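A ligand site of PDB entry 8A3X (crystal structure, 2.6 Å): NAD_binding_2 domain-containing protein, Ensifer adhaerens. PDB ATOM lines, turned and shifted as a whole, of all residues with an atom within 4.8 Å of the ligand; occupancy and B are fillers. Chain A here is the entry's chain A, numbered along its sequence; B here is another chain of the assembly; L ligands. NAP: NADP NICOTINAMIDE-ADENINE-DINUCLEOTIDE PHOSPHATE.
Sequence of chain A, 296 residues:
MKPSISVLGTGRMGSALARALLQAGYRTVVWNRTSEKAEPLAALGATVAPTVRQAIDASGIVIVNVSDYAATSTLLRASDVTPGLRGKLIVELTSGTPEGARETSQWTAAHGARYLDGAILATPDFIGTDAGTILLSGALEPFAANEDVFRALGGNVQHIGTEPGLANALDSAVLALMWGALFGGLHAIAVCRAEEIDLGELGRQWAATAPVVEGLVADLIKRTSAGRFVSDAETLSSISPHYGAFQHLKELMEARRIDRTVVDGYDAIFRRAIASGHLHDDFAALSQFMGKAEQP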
ATOM      1  N   GLY A   9      15.097 -12.092   6.604  1.00  0.00           N
ATOM      2  CA  GLY A   9      13.995 -11.412   7.295  1.00  0.00           C
ATOM      3  C   GLY A   9      12.782 -12.322   7.413  1.00  0.00           C
ATOM      4  O   GLY A   9      12.104 -12.581   6.374  1.00  0.00           O
ATOM      5  N   THR A  10      12.528 -12.803   8.629  1.00  0.00           N
ATOM      6  CA  THR A  10      11.357 -13.641   8.966  1.00  0.00           C
ATOM      7  C   THR A  10      10.387 -12.783   9.787  1.00  0.00           C
ATOM      8  O   THR A  10      10.059 -13.187  10.924  1.00  0.00           O
ATOM      9  CB  THR A  10      11.818 -14.916   9.673  1.00  0.00           C
ATOM     10  OG1 THR A  10      12.272 -14.613  10.996  1.00  0.00           O
ATOM     11  CG2 THR A  10      12.934 -15.593   8.900  1.00  0.00           C
ATOM     12  N   GLY A  11       9.983 -11.636   9.220  1.00  0.00           N
ATOM     13  CA  GLY A  11       8.959 -10.731   9.794  1.00  0.00           C
ATOM     14  C   GLY A  11       7.571 -11.348   9.705  1.00  0.00           C
ATOM     15  O   GLY A  11       7.473 -12.591   9.743  1.00  0.00           O
ATOM     16  N   ARG A  12       6.536 -10.525   9.579  1.00  0.00           N
ATOM     17  CA  ARG A  12       5.146 -10.990   9.313  1.00  0.00           C
ATOM     18  C   ARG A  12       5.078 -11.416   7.837  1.00  0.00           C
ATOM     19  O   ARG A  12       4.753 -12.572   7.558  1.00  0.00           O
ATOM     20  CB  ARG A  12       4.132  -9.902   9.661  1.00  0.00           C
ATOM     21  CG  ARG A  12       2.721 -10.436   9.861  1.00  0.00           C
ATOM     22  CD  ARG A  12       1.839  -9.552  10.702  1.00  0.00           C
ATOM     23  NE  ARG A  12       2.091  -9.730  12.131  1.00  0.00           N
ATOM     24  CZ  ARG A  12       2.786  -8.887  12.908  1.00  0.00           C
ATOM     25  NH1 ARG A  12       3.315  -7.779  12.404  1.00  0.00           N
ATOM     26  NH2 ARG A  12       2.950  -9.177  14.187  1.00  0.00           N
ATOM     27  N   MET A  13       5.376 -10.484   6.937  1.00  0.00           N
ATOM     28  CA  MET A  13       5.806 -10.755   5.555  1.00  0.00           C
ATOM     29  C   MET A  13       7.201 -11.369   5.640  1.00  0.00           C
ATOM     30  O   MET A  13       7.869 -11.197   6.688  1.00  0.00           O
ATOM     31  CB  MET A  13       5.856  -9.457   4.741  1.00  0.00           C
ATOM     32  CG  MET A  13       6.089  -9.656   3.270  1.00  0.00           C
ATOM     33  SD  MET A  13       4.638 -10.382   2.471  1.00  0.00           S
ATOM     34  CE  MET A  13       3.563  -8.957   2.421  1.00  0.00           C
ATOM     35  N   TRP A  31      17.166 -16.778   7.239  1.00  0.00           N
ATOM     36  CA  TRP A  31      17.927 -16.103   8.308  1.00  0.00           C
ATOM     37  C   TRP A  31      17.102 -14.935   8.829  1.00  0.00           C
ATOM     38  O   TRP A  31      16.295 -14.369   8.065  1.00  0.00           O
ATOM     39  CB  TRP A  31      19.312 -15.629   7.812  1.00  0.00           C
ATOM     40  CG  TRP A  31      20.081 -14.847   8.833  1.00  0.00           C
ATOM     41  CD1 TRP A  31      20.941 -15.323   9.777  1.00  0.00           C
ATOM     42  CD2 TRP A  31      20.046 -13.420   8.999  1.00  0.00           C
ATOM     43  NE1 TRP A  31      21.450 -14.293  10.530  1.00  0.00           N
ATOM     44  CE2 TRP A  31      20.914 -13.109  10.075  1.00  0.00           C
ATOM     45  CE3 TRP A  31      19.361 -12.375   8.356  1.00  0.00           C
ATOM     46  CZ2 TRP A  31      21.110 -11.802  10.520  1.00  0.00           C
ATOM     47  CZ3 TRP A  31      19.570 -11.084   8.786  1.00  0.00           C
ATOM     48  CH2 TRP A  31      20.422 -10.804   9.855  1.00  0.00           C
ATOM     49  N   ASN A  32      17.305 -14.603  10.105  1.00  0.00           N
ATOM     50  CA  ASN A  32      16.762 -13.396  10.759  1.00  0.00           C
ATOM     51  C   ASN A  32      17.674 -13.077  11.943  1.00  0.00           C
ATOM     52  O   ASN A  32      18.002 -14.024  12.688  1.00  0.00           O
ATOM     53  CB  ASN A  32      15.319 -13.620  11.204  1.00  0.00           C
ATOM     54  CG  ASN A  32      14.601 -12.325  11.503  1.00  0.00           C
ATOM     55  OD1 ASN A  32      14.600 -11.414  10.682  1.00  0.00           O
ATOM     56  ND2 ASN A  32      13.991 -12.221  12.673  1.00  0.00           N
ATOM     57  N   ARG A  33      18.102 -11.813  12.115  1.00  0.00           N
ATOM     58  CA  ARG A  33      18.660 -11.373  13.420  1.00  0.00           C
ATOM     59  C   ARG A  33      17.506 -11.498  14.388  1.00  0.00           C
ATOM     60  O   ARG A  33      16.361 -11.319  13.931  1.00  0.00           O
ATOM     61  CB  ARG A  33      19.261  -9.964  13.372  1.00  0.00           C
ATOM     62  CG  ARG A  33      18.273  -8.864  12.997  1.00  0.00           C
ATOM     63  CD  ARG A  33      18.508  -7.630  13.856  1.00  0.00           C
ATOM     64  NE  ARG A  33      17.554  -6.581  13.566  1.00  0.00           N
ATOM     65  CZ  ARG A  33      17.222  -5.603  14.396  1.00  0.00           C
ATOM     66  NH1 ARG A  33      17.778  -5.527  15.600  1.00  0.00           N
ATOM     67  NH2 ARG A  33      16.349  -4.687  14.034  1.00  0.00           N
ATOM     68  N   THR A  34      17.752 -11.840  15.655  1.00  0.00           N
ATOM     69  CA  THR A  34      16.690 -12.365  16.552  1.00  0.00           C
ATOM     70  C   THR A  34      16.184 -13.655  15.883  1.00  0.00           C
ATOM     71  O   THR A  34      15.105 -13.635  15.264  1.00  0.00           O
ATOM     72  CB  THR A  34      15.639 -11.287  16.883  1.00  0.00           C
ATOM     73  OG1 THR A  34      14.714 -11.074  15.807  1.00  0.00           O
ATOM     74  CG2 THR A  34      16.242  -9.943  17.247  1.00  0.00           C
ATOM     75  N   LYS A  37      12.636 -15.652  16.118  1.00  0.00           N
ATOM     76  CA  LYS A  37      11.453 -15.269  15.277  1.00  0.00           C
ATOM     77  C   LYS A  37      11.385 -16.153  14.022  1.00  0.00           C
ATOM     78  O   LYS A  37      10.325 -16.205  13.406  1.00  0.00           O
ATOM     79  CB  LYS A  37      11.480 -13.771  14.939  1.00  0.00           C
ATOM     80  N   ASN A  65      13.719  -9.137   2.712  1.00  0.00           N
ATOM     81  CA  ASN A  65      12.425  -8.618   3.215  1.00  0.00           C
ATOM     82  C   ASN A  65      12.550  -8.177   4.682  1.00  0.00           C
ATOM     83  O   ASN A  65      12.007  -8.859   5.586  1.00  0.00           O
ATOM     84  CB  ASN A  65      11.322  -9.647   2.998  1.00  0.00           C
ATOM     85  CG  ASN A  65       9.983  -8.989   3.146  1.00  0.00           C
ATOM     86  OD1 ASN A  65       9.642  -8.105   2.355  1.00  0.00           O
ATOM     87  ND2 ASN A  65       9.258  -9.360   4.189  1.00  0.00           N
ATOM     88  N   VAL A  66      13.209  -7.029   4.882  1.00  0.00           N
ATOM     89  CA  VAL A  66      13.583  -6.413   6.191  1.00  0.00           C
ATOM     90  C   VAL A  66      13.076  -4.969   6.215  1.00  0.00           C
ATOM     91  O   VAL A  66      12.422  -4.556   5.225  1.00  0.00           O
ATOM     92  CB  VAL A  66      15.109  -6.486   6.385  1.00  0.00           C
ATOM     93  CG1 VAL A  66      15.566  -7.919   6.616  1.00  0.00           C
ATOM     94  CG2 VAL A  66      15.868  -5.886   5.211  1.00  0.00           C
ATOM     95  N   SER A  67      13.365  -4.209   7.277  1.00  0.00           N
ATOM     96  CA  SER A  67      12.823  -2.840   7.529  1.00  0.00           C
ATOM     97  C   SER A  67      13.051  -1.938   6.306  1.00  0.00           C
ATOM     98  O   SER A  67      12.046  -1.522   5.710  1.00  0.00           O
ATOM     99  CB  SER A  67      13.391  -2.235   8.781  1.00  0.00           C
ATOM    100  OG  SER A  67      14.802  -2.145   8.709  1.00  0.00           O
ATOM    101  N   ALA A  71      19.212  -1.435   6.110  1.00  0.00           N
ATOM    102  CA  ALA A  71      19.376  -2.715   6.846  1.00  0.00           C
ATOM    103  C   ALA A  71      19.834  -3.808   5.872  1.00  0.00           C
ATOM    104  O   ALA A  71      20.771  -4.546   6.235  1.00  0.00           O
ATOM    105  CB  ALA A  71      18.120  -3.090   7.563  1.00  0.00           C
ATOM    106  N   LEU A  75      23.583  -5.922   5.882  1.00  0.00           N
ATOM    107  CA  LEU A  75      23.632  -7.408   5.842  1.00  0.00           C
ATOM    108  C   LEU A  75      24.490  -7.880   4.668  1.00  0.00           C
ATOM    109  O   LEU A  75      25.247  -8.831   4.855  1.00  0.00           O
ATOM    110  CB  LEU A  75      22.226  -7.986   5.695  1.00  0.00           C
ATOM    111  CG  LEU A  75      21.273  -7.753   6.852  1.00  0.00           C
ATOM    112  CD1 LEU A  75      19.964  -8.471   6.578  1.00  0.00           C
ATOM    113  CD2 LEU A  75      21.894  -8.212   8.160  1.00  0.00           C
ATOM    114  N   LEU A  93      12.720  -7.238  -1.848  1.00  0.00           N
ATOM    115  CA  LEU A  93      11.251  -7.127  -1.710  1.00  0.00           C
ATOM    116  C   LEU A  93      10.925  -6.248  -0.507  1.00  0.00           C
ATOM    117  O   LEU A  93       9.745  -6.209  -0.108  1.00  0.00           O
ATOM    118  CB  LEU A  93      10.667  -8.534  -1.558  1.00  0.00           C
ATOM    119  CG  LEU A  93       9.913  -9.072  -2.771  1.00  0.00           C
ATOM    120  CD1 LEU A  93      10.625  -8.713  -4.059  1.00  0.00           C
ATOM    121  CD2 LEU A  93       9.739 -10.589  -2.668  1.00  0.00           C
ATOM    122  N   THR A  94      11.922  -5.581   0.066  1.00  0.00           N
ATOM    123  CA  THR A  94      11.733  -4.618   1.186  1.00  0.00           C
ATOM    124  C   THR A  94      11.303  -3.283   0.559  1.00  0.00           C
ATOM    125  O   THR A  94      11.664  -3.032  -0.619  1.00  0.00           O
ATOM    126  CB  THR A  94      12.989  -4.504   2.072  1.00  0.00           C
ATOM    127  OG1 THR A  94      13.819  -3.478   1.548  1.00  0.00           O
ATOM    128  CG2 THR A  94      13.806  -5.766   2.182  1.00  0.00           C
ATOM    129  N   SER A  95      10.530  -2.479   1.295  1.00  0.00           N
ATOM    130  CA  SER A  95      10.011  -1.178   0.811  1.00  0.00           C
ATOM    131  C   SER A  95      11.168  -0.185   0.741  1.00  0.00           C
ATOM    132  O   SER A  95      11.939  -0.117   1.712  1.00  0.00           O
ATOM    133  CB  SER A  95       8.875  -0.679   1.684  1.00  0.00           C
ATOM    134  OG  SER A  95       7.770  -1.565   1.638  1.00  0.00           O
ATOM    135  N   ILE A 120       5.875  -5.569  -2.937  1.00  0.00           N
ATOM    136  CA  ILE A 120       4.758  -6.493  -2.584  1.00  0.00           C
ATOM    137  C   ILE A 120       3.490  -5.648  -2.369  1.00  0.00           C
ATOM    138  O   ILE A 120       3.375  -4.989  -1.321  1.00  0.00           O
ATOM    139  CB  ILE A 120       5.085  -7.300  -1.312  1.00  0.00           C
ATOM    140  CG1 ILE A 120       6.458  -7.985  -1.373  1.00  0.00           C
ATOM    141  CG2 ILE A 120       3.983  -8.298  -1.014  1.00  0.00           C
ATOM    142  CD1 ILE A 120       6.946  -8.486  -0.030  1.00  0.00           C
ATOM    143  N   ALA A 122       0.406  -6.421  -1.492  1.00  0.00           N
ATOM    144  CA  ALA A 122      -0.371  -7.518  -0.892  1.00  0.00           C
ATOM    145  C   ALA A 122       0.012  -7.689   0.574  1.00  0.00           C
ATOM    146  O   ALA A 122       1.165  -7.472   0.926  1.00  0.00           O
ATOM    147  CB  ALA A 122      -0.109  -8.791  -1.648  1.00  0.00           C
ATOM    148  N   THR A 123      -0.957  -8.044   1.399  1.00  0.00           N
ATOM    149  CA  THR A 123      -0.775  -8.369   2.824  1.00  0.00           C
ATOM    150  C   THR A 123      -0.396  -9.845   2.900  1.00  0.00           C
ATOM    151  O   THR A 123      -0.542 -10.550   1.908  1.00  0.00           O
ATOM    152  CB  THR A 123      -2.045  -7.981   3.597  1.00  0.00           C
ATOM    153  OG1 THR A 123      -3.176  -8.418   2.838  1.00  0.00           O
ATOM    154  CG2 THR A 123      -2.099  -6.487   3.842  1.00  0.00           C
ATOM    155  N   PRO A 124       0.125 -10.341   4.049  1.00  0.00           N
ATOM    156  CA  PRO A 124       0.501 -11.744   4.225  1.00  0.00           C
ATOM    157  C   PRO A 124      -0.496 -12.773   3.656  1.00  0.00           C
ATOM    158  O   PRO A 124      -0.074 -13.689   2.942  1.00  0.00           O
ATOM    159  CB  PRO A 124       0.542 -11.910   5.759  1.00  0.00           C
ATOM    160  CG  PRO A 124       0.952 -10.534   6.264  1.00  0.00           C
ATOM    161  CD  PRO A 124       0.427  -9.546   5.253  1.00  0.00           C
ATOM    162  N   LEU B 236      -2.276  -8.574   9.737  1.00  0.00           N
ATOM    163  CA  LEU B 236      -1.611  -8.613   8.424  1.00  0.00           C
ATOM    164  C   LEU B 236      -0.594  -7.477   8.315  1.00  0.00           C
ATOM    165  O   LEU B 236       0.244  -7.530   7.394  1.00  0.00           O
ATOM    166  CB  LEU B 236      -2.603  -8.604   7.239  1.00  0.00           C
ATOM    167  CG  LEU B 236      -3.992  -7.989   7.398  1.00  0.00           C
ATOM    168  CD1 LEU B 236      -4.989  -9.022   7.876  1.00  0.00           C
ATOM    169  CD2 LEU B 236      -3.989  -6.742   8.288  1.00  0.00           C
ATOM    170  N   SER B 237      -0.628  -6.493   9.222  1.00  0.00           N
ATOM    171  CA  SER B 237       0.239  -5.289   9.161  1.00  0.00           C
ATOM    172  C   SER B 237       0.455  -4.718  10.559  1.00  0.00           C
ATOM    173  O   SER B 237      -0.525  -4.605  11.275  1.00  0.00           O
ATOM    174  CB  SER B 237      -0.355  -4.244   8.231  1.00  0.00           C
ATOM    175  OG  SER B 237       0.582  -3.218   7.984  1.00  0.00           O
ATOM    176  N   SER B 238       1.705  -4.405  10.924  1.00  0.00           N
ATOM    177  CA  SER B 238       2.043  -3.651  12.156  1.00  0.00           C
ATOM    178  C   SER B 238       2.396  -2.209  11.764  1.00  0.00           C
ATOM    179  O   SER B 238       2.473  -1.918  10.560  1.00  0.00           O
ATOM    180  CB  SER B 238       3.120  -4.311  12.977  1.00  0.00           C
ATOM    181  OG  SER B 238       4.241  -4.610  12.167  1.00  0.00           O
ATOM    182  N   SER B 240       5.123  -0.360  12.405  1.00  0.00           N
ATOM    183  CA  SER B 240       6.559  -0.252  12.019  1.00  0.00           C
ATOM    184  C   SER B 240       6.699  -0.179  10.490  1.00  0.00           C
ATOM    185  O   SER B 240       7.180   0.826   9.973  1.00  0.00           O
ATOM    186  CB  SER B 240       7.357  -1.386  12.626  1.00  0.00           C
ATOM    187  OG  SER B 240       8.579  -1.580  11.941  1.00  0.00           O
ATOM    188  N   PRO B 241       6.289  -1.213   9.729  1.00  0.00           N
ATOM    189  CA  PRO B 241       6.504  -1.217   8.280  1.00  0.00           C
ATOM    190  C   PRO B 241       5.730  -0.110   7.563  1.00  0.00           C
ATOM    191  O   PRO B 241       6.217   0.411   6.577  1.00  0.00           O
ATOM    192  CB  PRO B 241       5.998  -2.592   7.818  1.00  0.00           C
ATOM    193  CG  PRO B 241       5.048  -3.032   8.924  1.00  0.00           C
ATOM    194  CD  PRO B 241       5.638  -2.442  10.190  1.00  0.00           C
ATOM    195  N   ALA B 245       7.717   2.626   5.313  1.00  0.00           N
ATOM    196  CA  ALA B 245       7.325   2.834   3.898  1.00  0.00           C
ATOM    197  C   ALA B 245       6.820   4.263   3.694  1.00  0.00           C
ATOM    198  O   ALA B 245       6.977   4.810   2.567  1.00  0.00           O
ATOM    199  CB  ALA B 245       6.273   1.830   3.522  1.00  0.00           C
ATOM    200  N   HIS B 280       5.267  -1.883  17.086  1.00  0.00           N
ATOM    201  CA  HIS B 280       5.114  -3.243  16.499  1.00  0.00           C
ATOM    202  C   HIS B 280       3.736  -3.815  16.863  1.00  0.00           C
ATOM    203  O   HIS B 280       3.608  -5.050  16.956  1.00  0.00           O
ATOM    204  CB  HIS B 280       6.256  -4.185  16.949  1.00  0.00           C
ATOM    205  CG  HIS B 280       7.617  -3.751  16.532  1.00  0.00           C
ATOM    206  ND1 HIS B 280       7.974  -3.616  15.197  1.00  0.00           N
ATOM    207  CD2 HIS B 280       8.705  -3.402  17.246  1.00  0.00           C
ATOM    208  CE1 HIS B 280       9.214  -3.180  15.116  1.00  0.00           C
ATOM    209  NE2 HIS B 280       9.698  -3.051  16.360  1.00  0.00           N
HETATM  210  PA  NAP L   1       8.046  -6.832  10.654  1.00  0.00           P
HETATM  211  O1A NAP L   1       7.197  -8.027  10.947  1.00  0.00           O
HETATM  212  O2A NAP L   1       8.008  -5.680  11.613  1.00  0.00           O
HETATM  213  O5B NAP L   1       9.557  -7.365  10.476  1.00  0.00           O
HETATM  214  C5B NAP L   1      10.670  -6.619   9.901  1.00  0.00           C
HETATM  215  C4B NAP L   1      11.786  -7.587   9.540  1.00  0.00           C
HETATM  216  O4B NAP L   1      12.992  -6.840   9.243  1.00  0.00           O
HETATM  217  C3B NAP L   1      12.210  -8.597  10.621  1.00  0.00           C
HETATM  218  O3B NAP L   1      12.651  -9.817  10.025  1.00  0.00           O
HETATM  219  C2B NAP L   1      13.334  -7.849  11.314  1.00  0.00           C
HETATM  220  O2B NAP L   1      14.297  -8.631  12.015  1.00  0.00           O
HETATM  221  C1B NAP L   1      14.026  -7.263  10.103  1.00  0.00           C
HETATM  222  N9A NAP L   1      14.853  -6.113  10.447  1.00  0.00           N
HETATM  223  C8A NAP L   1      14.415  -4.888  10.898  1.00  0.00           C
HETATM  224  N7A NAP L   1      15.391  -4.055  11.128  1.00  0.00           N
HETATM  225  C5A NAP L   1      16.544  -4.780  10.836  1.00  0.00           C
HETATM  226  C6A NAP L   1      17.912  -4.450  10.892  1.00  0.00           C
HETATM  227  N6A NAP L   1      18.340  -3.248  11.272  1.00  0.00           N
HETATM  228  N1A NAP L   1      18.810  -5.388  10.540  1.00  0.00           N
HETATM  229  C2A NAP L   1      18.354  -6.589  10.161  1.00  0.00           C
HETATM  230  N3A NAP L   1      17.093  -7.010  10.059  1.00  0.00           N
HETATM  231  C4A NAP L   1      16.224  -6.059  10.422  1.00  0.00           C
HETATM  232  O3  NAP L   1       7.757  -6.259   9.186  1.00  0.00           O
HETATM  233  PN  NAP L   1       7.064  -6.899   7.900  1.00  0.00           P
HETATM  234  O1N NAP L   1       5.606  -6.697   8.116  1.00  0.00           O
HETATM  235  O2N NAP L   1       7.585  -8.272   7.655  1.00  0.00           O
HETATM  236  O5D NAP L   1       7.568  -5.949   6.724  1.00  0.00           O
HETATM  237  C5D NAP L   1       8.582  -6.531   5.870  1.00  0.00           C
HETATM  238  C4D NAP L   1       8.861  -5.639   4.682  1.00  0.00           C
HETATM  239  O4D NAP L   1       7.821  -5.845   3.705  1.00  0.00           O
HETATM  240  C3D NAP L   1       8.936  -4.118   4.924  1.00  0.00           C
HETATM  241  O3D NAP L   1       9.934  -3.472   4.127  1.00  0.00           O
HETATM  242  C2D NAP L   1       7.574  -3.622   4.435  1.00  0.00           C
HETATM  243  O2D NAP L   1       7.692  -2.277   3.987  1.00  0.00           O
HETATM  244  C1D NAP L   1       7.279  -4.610   3.315  1.00  0.00           C
HETATM  245  N1N NAP L   1       5.832  -4.839   3.107  1.00  0.00           N
HETATM  246  C2N NAP L   1       5.086  -5.445   4.087  1.00  0.00           C
HETATM  247  C3N NAP L   1       3.784  -5.823   3.818  1.00  0.00           C
HETATM  248  C7N NAP L   1       2.877  -6.357   4.888  1.00  0.00           C
HETATM  249  O7N NAP L   1       1.731  -6.681   4.583  1.00  0.00           O
HETATM  250  N7N NAP L   1       3.358  -6.452   6.116  1.00  0.00           N
HETATM  251  C4N NAP L   1       3.294  -5.694   2.537  1.00  0.00           C
HETATM  252  C5N NAP L   1       4.057  -5.066   1.575  1.00  0.00           C
HETATM  253  C6N NAP L   1       5.272  -4.535   1.925  1.00  0.00           C
HETATM  254  P2B NAP L   1      14.152  -8.453  13.622  1.00  0.00           P
HETATM  255  O1X NAP L   1      13.183  -9.574  13.967  1.00  0.00           O
HETATM  256  O2X NAP L   1      15.494  -8.628  14.308  1.00  0.00           O
HETATM  257  O3X NAP L   1      13.583  -7.075  13.882  1.00  0.00           O
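The backbone carbonyl oxygen of Thr 34 is in hydrogen-bond range of the side-chain amide nitrogen of Asn 32, 3.2 Å away. The backbone NH of Thr 10 sits at hydrogen-bond distance from the side-chain amide oxygen of Asn 32. The guanidinium group (NH1) of Arg 12 lies within hydrogen-bond range of the side-chain hydroxyl (OG) of Ser 238 of chain B (3.3 Å). The backbone carbonyl oxygen (O) of Met 13 sits close to the side-chain amide nitrogen (ND2) of Asn 65. The backbone carbonyl oxygen (O) of Leu 93 sits close to the side-chain amide oxygen (OD1) of Asn 65 (3.1 Å). The side-chain hydroxyl (OG1) of Thr 10 lies within hydrogen-bond range of the backbone carbonyl oxygen (O) of Lys 37, at 3.5 Å. N of Gly 9 sits at hydrogen-bond distance from O of Trp 31, at 3.0 Å.
N of Ser 95 lies within hydrogen-bond range of O3D of the ligand, 3.1 Å away. OG of Ser 95 lies within hydrogen-bond range of O2D of the ligand. OD1 of Asn 32 lies within hydrogen-bond range of O3B of the ligand (2.6 Å). The side-chain hydroxyl of Thr 34 is in hydrogen-bond range of an oxygen (O1X) of the ligand (2.8 Å). O2X of the ligand sits close to O of Arg 33 (2.9 Å). NE of Arg 33 is in salt-bridge range of O2X of the ligand, 3.0 Å away. The backbone NH (N) of Arg 12 sits at hydrogen-bond distance from an oxygen (O1A) of the ligand. O3D of the ligand sits at hydrogen-bond distance from O of Val 66 (2.9 Å). An oxygen (O2N) of the ligand lies within hydrogen-bond range of the backbone NH of Met 13. O2N of the ligand lies close to O of Met 13, at 3.1 Å. An oxygen (O4B) of the ligand is in hydrogen-bond range of the backbone NH (N) of Ser 67. The backbone carbonyl oxygen (O) of Ser 67 lies within hydrogen-bond range of an oxygen (O3D) of the ligand, at 3.3 Å. A nitrogen (N7A) of the ligand is in hydrogen-bond range of the side-chain hydroxyl (OG) of Ser 67, at 3.1 Å. The side-chain amide oxygen (OD1) of Asn 65 sits close to an oxygen (O4D) of the ligand. An oxygen (O3B) of the ligand lies within hydrogen-bond range of the backbone NH of Thr 10, at 3.3 Å. The backbone NH of Gly 11 lies within hydrogen-bond range of an oxygen (O3B) of the ligand (3.3 Å).
The backbone carbonyl oxygen (O) of Leu 236 of chain B lies close to an oxygen (O7N) of the ligand, 3.3 Å away. Merely in contact with the ligand: Ile 120, Ala 122, Pro 124, Gly 9, Thr 123, Ala 71, Thr 94, Pro 241 of chain B and Ser 238 of chain B. Of the 29 residues printed, 21 come within 4 Å of the ligand. The nearest printed residue that does not touch the ligand is His 280 of chain B (4.1 Å).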
